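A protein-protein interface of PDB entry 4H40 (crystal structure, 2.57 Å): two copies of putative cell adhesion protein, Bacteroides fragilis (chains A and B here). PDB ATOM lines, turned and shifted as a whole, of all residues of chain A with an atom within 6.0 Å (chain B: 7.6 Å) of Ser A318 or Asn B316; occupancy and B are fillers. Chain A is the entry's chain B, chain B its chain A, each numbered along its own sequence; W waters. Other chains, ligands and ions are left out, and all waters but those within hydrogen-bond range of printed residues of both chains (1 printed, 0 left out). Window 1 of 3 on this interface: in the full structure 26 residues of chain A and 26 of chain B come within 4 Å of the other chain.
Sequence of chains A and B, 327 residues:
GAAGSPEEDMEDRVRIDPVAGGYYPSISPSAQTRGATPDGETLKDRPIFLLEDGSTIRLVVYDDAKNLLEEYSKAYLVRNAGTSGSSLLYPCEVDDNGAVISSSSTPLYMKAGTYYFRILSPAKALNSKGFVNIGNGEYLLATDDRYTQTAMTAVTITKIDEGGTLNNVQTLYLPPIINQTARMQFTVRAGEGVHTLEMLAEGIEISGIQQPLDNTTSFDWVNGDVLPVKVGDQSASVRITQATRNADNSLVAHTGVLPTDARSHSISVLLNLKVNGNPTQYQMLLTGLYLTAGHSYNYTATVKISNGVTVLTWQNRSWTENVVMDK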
ATOM      1  N   TRP A 314     -26.087 -32.347  38.875  1.00  0.00           N
ATOM      2  CA  TRP A 314     -26.944 -31.208  38.670  1.00  0.00           C
ATOM      3  C   TRP A 314     -27.468 -31.147  37.257  1.00  0.00           C
ATOM      4  O   TRP A 314     -27.017 -31.846  36.368  1.00  0.00           O
ATOM      5  CB  TRP A 314     -26.319 -29.872  39.101  1.00  0.00           C
ATOM      6  CG  TRP A 314     -25.282 -29.327  38.189  1.00  0.00           C
ATOM      7  CD1 TRP A 314     -25.444 -28.351  37.248  1.00  0.00           C
ATOM      8  CD2 TRP A 314     -23.893 -29.645  38.208  1.00  0.00           C
ATOM      9  NE1 TRP A 314     -24.238 -28.050  36.665  1.00  0.00           N
ATOM     10  CE2 TRP A 314     -23.265 -28.845  37.221  1.00  0.00           C
ATOM     11  CE3 TRP A 314     -23.113 -30.566  38.939  1.00  0.00           C
ATOM     12  CZ2 TRP A 314     -21.881 -28.932  36.948  1.00  0.00           C
ATOM     13  CZ3 TRP A 314     -21.749 -30.636  38.684  1.00  0.00           C
ATOM     14  CH2 TRP A 314     -21.148 -29.842  37.688  1.00  0.00           C
ATOM     15  N   GLN A 315     -28.513 -30.360  37.120  1.00  0.00           N
ATOM     16  CA  GLN A 315     -29.224 -30.052  35.914  1.00  0.00           C
ATOM     17  C   GLN A 315     -29.630 -28.584  35.944  1.00  0.00           C
ATOM     18  O   GLN A 315     -29.813 -27.967  37.015  1.00  0.00           O
ATOM     19  CB  GLN A 315     -30.424 -30.977  35.734  1.00  0.00           C
ATOM     20  CG  GLN A 315     -31.363 -31.055  36.941  1.00  0.00           C
ATOM     21  CD  GLN A 315     -32.194 -32.325  36.971  1.00  0.00           C
ATOM     22  OE1 GLN A 315     -31.996 -33.272  36.182  1.00  0.00           O
ATOM     23  NE2 GLN A 315     -33.126 -32.381  37.919  1.00  0.00           N
ATOM     24  N   ASN A 316     -29.719 -28.022  34.758  1.00  0.00           N
ATOM     25  CA  ASN A 316     -30.119 -26.657  34.548  1.00  0.00           C
ATOM     26  C   ASN A 316     -30.409 -26.481  33.068  1.00  0.00           C
ATOM     27  O   ASN A 316     -29.802 -27.161  32.232  1.00  0.00           O
ATOM     28  CB  ASN A 316     -29.041 -25.683  35.056  1.00  0.00           C
ATOM     29  CG  ASN A 316     -27.897 -25.447  34.109  1.00  0.00           C
ATOM     30  OD1 ASN A 316     -27.168 -26.363  33.735  1.00  0.00           O
ATOM     31  ND2 ASN A 316     -27.774 -24.210  33.642  1.00  0.00           N
ATOM     32  N   ARG A 317     -31.363 -25.595  32.750  1.00  0.00           N
ATOM     33  CA  ARG A 317     -31.731 -25.288  31.373  1.00  0.00           C
ATOM     34  C   ARG A 317     -30.784 -24.214  30.863  1.00  0.00           C
ATOM     35  O   ARG A 317     -30.448 -23.302  31.609  1.00  0.00           O
ATOM     36  CB  ARG A 317     -33.209 -24.844  31.280  1.00  0.00           C
ATOM     37  CG  ARG A 317     -33.761 -24.747  29.856  1.00  0.00           C
ATOM     38  CD  ARG A 317     -35.151 -25.321  29.757  1.00  0.00           C
ATOM     39  NE  ARG A 317     -35.106 -26.757  29.485  1.00  0.00           N
ATOM     40  CZ  ARG A 317     -35.166 -27.288  28.267  1.00  0.00           C
ATOM     41  NH1 ARG A 317     -35.315 -26.510  27.203  1.00  0.00           N
ATOM     42  NH2 ARG A 317     -35.095 -28.601  28.107  1.00  0.00           N
ATOM     43  N   SER A 318     -30.343 -24.332  29.601  1.00  0.00           N
ATOM     44  CA  SER A 318     -29.463 -23.349  28.979  1.00  0.00           C
ATOM     45  C   SER A 318     -30.077 -22.843  27.648  1.00  0.00           C
ATOM     46  O   SER A 318     -30.791 -23.588  26.989  1.00  0.00           O
ATOM     47  CB  SER A 318     -28.073 -23.940  28.777  1.00  0.00           C
ATOM     48  OG  SER A 318     -27.337 -23.861  29.989  1.00  0.00           O
ATOM     49  N   TRP A 319     -29.861 -21.551  27.312  1.00  0.00           N
ATOM     50  CA  TRP A 319     -30.401 -20.857  26.126  1.00  0.00           C
ATOM     51  C   TRP A 319     -29.227 -20.201  25.404  1.00  0.00           C
ATOM     52  O   TRP A 319     -28.388 -19.609  26.088  1.00  0.00           O
ATOM     53  CB  TRP A 319     -31.497 -19.782  26.529  1.00  0.00           C
ATOM     54  CG  TRP A 319     -32.487 -20.239  27.583  1.00  0.00           C
ATOM     55  CD1 TRP A 319     -32.231 -20.426  28.912  1.00  0.00           C
ATOM     56  CD2 TRP A 319     -33.853 -20.658  27.380  1.00  0.00           C
ATOM     57  NE1 TRP A 319     -33.338 -20.953  29.545  1.00  0.00           N
ATOM     58  CE2 TRP A 319     -34.343 -21.115  28.629  1.00  0.00           C
ATOM     59  CE3 TRP A 319     -34.720 -20.674  26.267  1.00  0.00           C
ATOM     60  CZ2 TRP A 319     -35.648 -21.608  28.793  1.00  0.00           C
ATOM     61  CZ3 TRP A 319     -36.004 -21.195  26.421  1.00  0.00           C
ATOM     62  CH2 TRP A 319     -36.457 -21.657  27.670  1.00  0.00           C
ATOM     63  N   THR A 320     -29.110 -20.360  24.059  1.00  0.00           N
ATOM     64  CA  THR A 320     -28.080 -19.670  23.272  1.00  0.00           C
ATOM     65  C   THR A 320     -28.662 -19.175  21.979  1.00  0.00           C
ATOM     66  O   THR A 320     -29.392 -19.905  21.307  1.00  0.00           O
ATOM     67  CB  THR A 320     -26.803 -20.476  22.970  1.00  0.00           C
ATOM     68  OG1 THR A 320     -27.088 -21.681  22.246  1.00  0.00           O
ATOM     69  CG2 THR A 320     -25.888 -20.653  24.177  1.00  0.00           C
ATOM     70  N   GLN B 283     -23.986 -22.593  19.621  1.00  0.00           N
ATOM     71  CA  GLN B 283     -22.945 -23.271  20.367  1.00  0.00           C
ATOM     72  C   GLN B 283     -23.418 -23.772  21.711  1.00  0.00           C
ATOM     73  O   GLN B 283     -23.912 -23.013  22.555  1.00  0.00           O
ATOM     74  CB  GLN B 283     -21.706 -22.403  20.556  1.00  0.00           C
ATOM     75  CG  GLN B 283     -20.682 -23.115  21.439  1.00  0.00           C
ATOM     76  CD  GLN B 283     -19.424 -22.347  21.572  1.00  0.00           C
ATOM     77  OE1 GLN B 283     -18.364 -22.821  21.166  1.00  0.00           O
ATOM     78  NE2 GLN B 283     -19.518 -21.141  22.130  1.00  0.00           N
ATOM     79  N   MET B 284     -23.208 -25.062  21.913  1.00  0.00           N
ATOM     80  CA  MET B 284     -23.431 -25.678  23.217  1.00  0.00           C
ATOM     81  C   MET B 284     -22.061 -25.871  23.791  1.00  0.00           C
ATOM     82  O   MET B 284     -21.156 -26.267  23.073  1.00  0.00           O
ATOM     83  CB  MET B 284     -24.199 -27.007  23.155  1.00  0.00           C
ATOM     84  CG  MET B 284     -25.554 -26.909  22.522  1.00  0.00           C
ATOM     85  SD  MET B 284     -26.281 -28.681  22.057  1.00  0.00           S
ATOM     86  CE  MET B 284     -26.568 -29.429  23.816  1.00  0.00           C
ATOM     87  N   LEU B 285     -21.877 -25.482  25.023  1.00  0.00           N
ATOM     88  CA  LEU B 285     -20.662 -25.719  25.764  1.00  0.00           C
ATOM     89  C   LEU B 285     -21.049 -26.659  26.889  1.00  0.00           C
ATOM     90  O   LEU B 285     -21.948 -26.335  27.683  1.00  0.00           O
ATOM     91  CB  LEU B 285     -20.054 -24.413  26.266  1.00  0.00           C
ATOM     92  CG  LEU B 285     -19.147 -23.691  25.306  1.00  0.00           C
ATOM     93  CD1 LEU B 285     -19.135 -22.190  25.606  1.00  0.00           C
ATOM     94  CD2 LEU B 285     -17.749 -24.286  25.333  1.00  0.00           C
ATOM     95  N   LEU B 286     -20.468 -27.877  26.899  1.00  0.00           N
ATOM     96  CA  LEU B 286     -20.833 -28.901  27.906  1.00  0.00           C
ATOM     97  C   LEU B 286     -19.686 -29.148  28.854  1.00  0.00           C
ATOM     98  O   LEU B 286     -18.562 -29.232  28.406  1.00  0.00           O
ATOM     99  CB  LEU B 286     -21.301 -30.243  27.290  1.00  0.00           C
ATOM    100  CG  LEU B 286     -22.172 -30.201  26.056  1.00  0.00           C
ATOM    101  CD1 LEU B 286     -22.138 -31.532  25.335  1.00  0.00           C
ATOM    102  CD2 LEU B 286     -23.595 -29.782  26.384  1.00  0.00           C
ATOM    103  N   THR B 287     -19.983 -29.302  30.161  1.00  0.00           N
ATOM    104  CA  THR B 287     -18.976 -29.499  31.204  1.00  0.00           C
ATOM    105  C   THR B 287     -19.514 -30.436  32.312  1.00  0.00           C
ATOM    106  O   THR B 287     -20.712 -30.736  32.347  1.00  0.00           O
ATOM    107  CB  THR B 287     -18.514 -28.120  31.718  1.00  0.00           C
ATOM    108  OG1 THR B 287     -17.312 -28.279  32.473  1.00  0.00           O
ATOM    109  CG2 THR B 287     -19.596 -27.373  32.502  1.00  0.00           C
ATOM    110  N   LEU B 289     -18.655 -33.593  32.700  1.00  0.00           N
ATOM    111  CA  LEU B 289     -18.849 -34.814  31.965  1.00  0.00           C
ATOM    112  C   LEU B 289     -17.642 -35.705  31.929  1.00  0.00           C
ATOM    113  O   LEU B 289     -16.577 -35.273  31.534  1.00  0.00           O
ATOM    114  CB  LEU B 289     -19.182 -34.420  30.532  1.00  0.00           C
ATOM    115  CG  LEU B 289     -20.619 -34.114  30.235  1.00  0.00           C
ATOM    116  CD1 LEU B 289     -20.771 -33.866  28.760  1.00  0.00           C
ATOM    117  CD2 LEU B 289     -21.524 -35.253  30.693  1.00  0.00           C
ATOM    118  N   TYR B 299     -28.460 -35.601  24.099  1.00  0.00           N
ATOM    119  CA  TYR B 299     -28.921 -34.250  24.242  1.00  0.00           C
ATOM    120  C   TYR B 299     -30.151 -34.017  23.401  1.00  0.00           C
ATOM    121  O   TYR B 299     -30.259 -34.506  22.275  1.00  0.00           O
ATOM    122  CB  TYR B 299     -27.774 -33.267  23.908  1.00  0.00           C
ATOM    123  CG  TYR B 299     -26.724 -33.279  25.007  1.00  0.00           C
ATOM    124  CD1 TYR B 299     -25.620 -34.134  24.938  1.00  0.00           C
ATOM    125  CD2 TYR B 299     -26.910 -32.549  26.181  1.00  0.00           C
ATOM    126  CE1 TYR B 299     -24.732 -34.257  26.011  1.00  0.00           C
ATOM    127  CE2 TYR B 299     -26.025 -32.651  27.248  1.00  0.00           C
ATOM    128  CZ  TYR B 299     -24.940 -33.510  27.164  1.00  0.00           C
ATOM    129  OH  TYR B 299     -24.082 -33.588  28.238  1.00  0.00           O
ATOM    130  N   THR B 300     -31.121 -33.331  24.020  1.00  0.00           N
ATOM    131  CA  THR B 300     -32.376 -32.920  23.424  1.00  0.00           C
ATOM    132  C   THR B 300     -32.388 -31.378  23.452  1.00  0.00           C
ATOM    133  O   THR B 300     -32.493 -30.760  24.525  1.00  0.00           O
ATOM    134  CB  THR B 300     -33.559 -33.601  24.104  1.00  0.00           C
ATOM    135  OG1 THR B 300     -33.250 -34.995  24.266  1.00  0.00           O
ATOM    136  CG2 THR B 300     -34.808 -33.489  23.282  1.00  0.00           C
ATOM    137  N   THR B 302     -33.894 -27.774  21.518  1.00  0.00           N
ATOM    138  CA  THR B 302     -35.086 -27.278  20.845  1.00  0.00           C
ATOM    139  C   THR B 302     -34.803 -25.933  20.223  1.00  0.00           C
ATOM    140  O   THR B 302     -34.316 -25.027  20.910  1.00  0.00           O
ATOM    141  CB  THR B 302     -36.270 -27.187  21.834  1.00  0.00           C
ATOM    142  OG1 THR B 302     -36.456 -28.468  22.450  1.00  0.00           O
ATOM    143  CG2 THR B 302     -37.580 -26.710  21.159  1.00  0.00           C
ATOM    144  N   VAL B 311     -33.641 -19.129  18.924  1.00  0.00           N
ATOM    145  CA  VAL B 311     -32.794 -19.615  20.025  1.00  0.00           C
ATOM    146  C   VAL B 311     -32.776 -21.133  20.096  1.00  0.00           C
ATOM    147  O   VAL B 311     -33.688 -21.800  19.614  1.00  0.00           O
ATOM    148  CB  VAL B 311     -33.132 -19.039  21.421  1.00  0.00           C
ATOM    149  CG1 VAL B 311     -32.601 -17.626  21.559  1.00  0.00           C
ATOM    150  CG2 VAL B 311     -34.624 -19.127  21.758  1.00  0.00           C
ATOM    151  N   LEU B 312     -31.744 -21.661  20.755  1.00  0.00           N
ATOM    152  CA  LEU B 312     -31.540 -23.063  21.050  1.00  0.00           C
ATOM    153  C   LEU B 312     -31.510 -23.215  22.542  1.00  0.00           C
ATOM    154  O   LEU B 312     -30.780 -22.497  23.232  1.00  0.00           O
ATOM    155  CB  LEU B 312     -30.261 -23.611  20.419  1.00  0.00           C
ATOM    156  CG  LEU B 312     -30.231 -25.135  20.291  1.00  0.00           C
ATOM    157  CD1 LEU B 312     -30.606 -25.560  18.910  1.00  0.00           C
ATOM    158  CD2 LEU B 312     -28.860 -25.710  20.670  1.00  0.00           C
ATOM    159  N   THR B 313     -32.350 -24.119  23.050  1.00  0.00           N
ATOM    160  CA  THR B 313     -32.432 -24.406  24.478  1.00  0.00           C
ATOM    161  C   THR B 313     -32.262 -25.896  24.723  1.00  0.00           C
ATOM    162  O   THR B 313     -32.750 -26.735  23.950  1.00  0.00           O
ATOM    163  CB  THR B 313     -33.739 -23.843  25.100  1.00  0.00           C
ATOM    164  OG1 THR B 313     -33.736 -24.033  26.521  1.00  0.00           O
ATOM    165  CG2 THR B 313     -35.011 -24.403  24.466  1.00  0.00           C
ATOM    166  N   TRP B 314     -31.544 -26.221  25.792  1.00  0.00           N
ATOM    167  CA  TRP B 314     -31.365 -27.610  26.168  1.00  0.00           C
ATOM    168  C   TRP B 314     -31.196 -27.734  27.668  1.00  0.00           C
ATOM    169  O   TRP B 314     -31.122 -26.728  28.377  1.00  0.00           O
ATOM    170  CB  TRP B 314     -30.180 -28.246  25.426  1.00  0.00           C
ATOM    171  CG  TRP B 314     -28.859 -27.793  25.947  1.00  0.00           C
ATOM    172  CD1 TRP B 314     -28.061 -28.444  26.841  1.00  0.00           C
ATOM    173  CD2 TRP B 314     -28.203 -26.568  25.636  1.00  0.00           C
ATOM    174  NE1 TRP B 314     -26.948 -27.695  27.112  1.00  0.00           N
ATOM    175  CE2 TRP B 314     -26.992 -26.547  26.364  1.00  0.00           C
ATOM    176  CE3 TRP B 314     -28.491 -25.499  24.760  1.00  0.00           C
ATOM    177  CZ2 TRP B 314     -26.075 -25.499  26.254  1.00  0.00           C
ATOM    178  CZ3 TRP B 314     -27.606 -24.436  24.690  1.00  0.00           C
ATOM    179  CH2 TRP B 314     -26.413 -24.443  25.424  1.00  0.00           C
ATOM    180  N   GLN B 315     -31.078 -28.981  28.143  1.00  0.00           N
ATOM    181  CA  GLN B 315     -30.889 -29.283  29.545  1.00  0.00           C
ATOM    182  C   GLN B 315     -29.514 -29.923  29.756  1.00  0.00           C
ATOM    183  O   GLN B 315     -29.110 -30.829  29.021  1.00  0.00           O
ATOM    184  CB  GLN B 315     -32.048 -30.184  30.042  1.00  0.00           C
ATOM    185  CG  GLN B 315     -32.109 -30.432  31.571  1.00  0.00           C
ATOM    186  CD  GLN B 315     -33.172 -29.660  32.326  1.00  0.00           C
ATOM    187  OE1 GLN B 315     -32.950 -29.193  33.455  1.00  0.00           O
ATOM    188  NE2 GLN B 315     -34.366 -29.555  31.756  1.00  0.00           N
ATOM    189  N   ASN B 316     -28.764 -29.373  30.721  1.00  0.00           N
ATOM    190  CA  ASN B 316     -27.468 -29.922  31.137  1.00  0.00           C
ATOM    191  C   ASN B 316     -27.671 -30.917  32.232  1.00  0.00           C
ATOM    192  O   ASN B 316     -28.483 -30.682  33.131  1.00  0.00           O
ATOM    193  CB  ASN B 316     -26.519 -28.848  31.670  1.00  0.00           C
ATOM    194  CG  ASN B 316     -26.193 -27.800  30.685  1.00  0.00           C
ATOM    195  OD1 ASN B 316     -26.769 -26.701  30.743  1.00  0.00           O
ATOM    196  ND2 ASN B 316     -25.319 -28.156  29.724  1.00  0.00           N
ATOM    197  N   ARG B 317     -26.930 -32.010  32.174  1.00  0.00           N
ATOM    198  CA  ARG B 317     -26.880 -33.021  33.211  1.00  0.00           C
ATOM    199  C   ARG B 317     -25.399 -33.284  33.420  1.00  0.00           C
ATOM    200  O   ARG B 317     -24.678 -33.658  32.491  1.00  0.00           O
ATOM    201  CB  ARG B 317     -27.723 -34.271  32.903  1.00  0.00           C
ATOM    202  N   SER B 318     -24.918 -32.872  34.582  1.00  0.00           N
ATOM    203  CA  SER B 318     -23.515 -33.011  34.972  1.00  0.00           C
ATOM    204  C   SER B 318     -23.447 -33.689  36.324  1.00  0.00           C
ATOM    205  O   SER B 318     -24.473 -33.907  36.944  1.00  0.00           O
ATOM    206  CB  SER B 318     -22.807 -31.652  35.006  1.00  0.00           C
ATOM    207  OG  SER B 318     -23.342 -30.634  34.166  1.00  0.00           O
HETATM  208  O   HOH W   1     -35.146 -28.834  24.894  1.00  0.00           O
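Among the printed residues, merely in contact across the chains: Trp A314 with Asn B316 (3.7 Å), Trp A314 with Arg B317 (3.4 Å), Gln A315 with Gln B315 (3.8 Å), Gln A315 with Asn B316 (2.9 Å), Asn A316 with Gln B315 (3.6 Å), Arg A317 with Trp B314 (3.4 Å), Arg A317 with Gln B315 (3.7 Å), Ser A318 with Leu B312 (3.9 Å), Trp A319 with Leu B312 (3.3 Å), Trp A319 with Thr B313 (3.5 Å), Thr A320 with Val B311 (3.6 Å) and Thr A320 with Trp B314 (3.7 Å).
O of Thr B287 lies within hydrogen-bond range of OG of Ser B318 (3.2 Å). The backbone carbonyl oxygen of Thr B313 lies within hydrogen-bond range of the backbone NH of Thr B302. The indole nitrogen (NE1) of Trp B314 lies close to the side-chain amide nitrogen (ND2) of Asn B316 (3.1 Å).
Water W1 lies within hydrogen-bond range of the side-chain hydroxyl of Thr B302, the guanidinium group of Arg A317, the backbone carbonyl oxygen of Thr B300 and the backbone carbonyl oxygen of Thr B313.
Trp A314 touches Asn B316, but with the chains exchanged Asn A316 does not touch Trp B314 (4.1 Å). Trp A314 touches Arg B317, and with the chains exchanged Arg A317 touches Trp B314. Gln A315 touches Asn B316, and with the chains exchanged Asn A316 touches Gln B315. Ser A318 touches Asn B316, but with the chains exchanged Asn A316 does not touch Ser B318 (5.8 Å). 5 positions are printed for both chains.
Of the printed residues of chain B, Trp A314 touches Asn B316 (3.7 Å), Arg B317 (3.4 Å) and Ser B318 (2.9 Å). Printed residues of chain B within 4 Å of Asn A316: Gln B315 (3.6 Å) and Asn B316 (2.9 Å). Of chain B, only Leu B312, Thr B313, Trp B314 and Asn B316 come within 4 Å of Ser A318. Of chain A, only Trp A314, Gln A315, Asn A316 and Ser A318 come within 4 Å of Asn B316. Printed residues of chain A within 4 Å of Ser B318: Trp A314. The nearest residue of chain B that does not touch Ser A318 is Gln B315 (4.9 Å).
Of the 17 printed residues of chain B, 9 touch a printed residue of chain A. Hydrophobic or aromatic side chains of chain B within 4 Å of the printed part of chain A: Val B311, Leu B312 and Trp B314. Among the printed residues, 20 pairs touch across the chains.
The backbone carbonyl oxygen (O) of Gln B283 lies within hydrogen-bond range of the side-chain hydroxyl (OG1) of Thr A320, at 3.5 Å. O of Leu B312 sits at hydrogen-bond distance from N of Thr A320, 2.8 Å away. The side-chain hydroxyl (OG1) of Thr B313 sits at hydrogen-bond distance from the guanidinium group (NH1) of Arg A317 (3.0 Å). The side-chain hydroxyl (OG1) of Thr B313 sits at hydrogen-bond distance from the backbone carbonyl oxygen (O) of Ser A318 (3.0 Å). The backbone carbonyl oxygen (O) of Trp B314 lies within hydrogen-bond range of the backbone NH (N) of Ser A318. The backbone carbonyl oxygen (O) of Asn A316 lies within hydrogen-bond range of the backbone NH (N) of Asn B316 (2.9 Å). The side-chain amide oxygen (OD1) of Asn B316 sits at hydrogen-bond distance from the side-chain hydroxyl (OG) of Ser A318 (3.0 Å). The backbone carbonyl oxygen (O) of Trp A314 sits at hydrogen-bond distance from the backbone NH (N) of Ser B318, 2.9 Å away.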
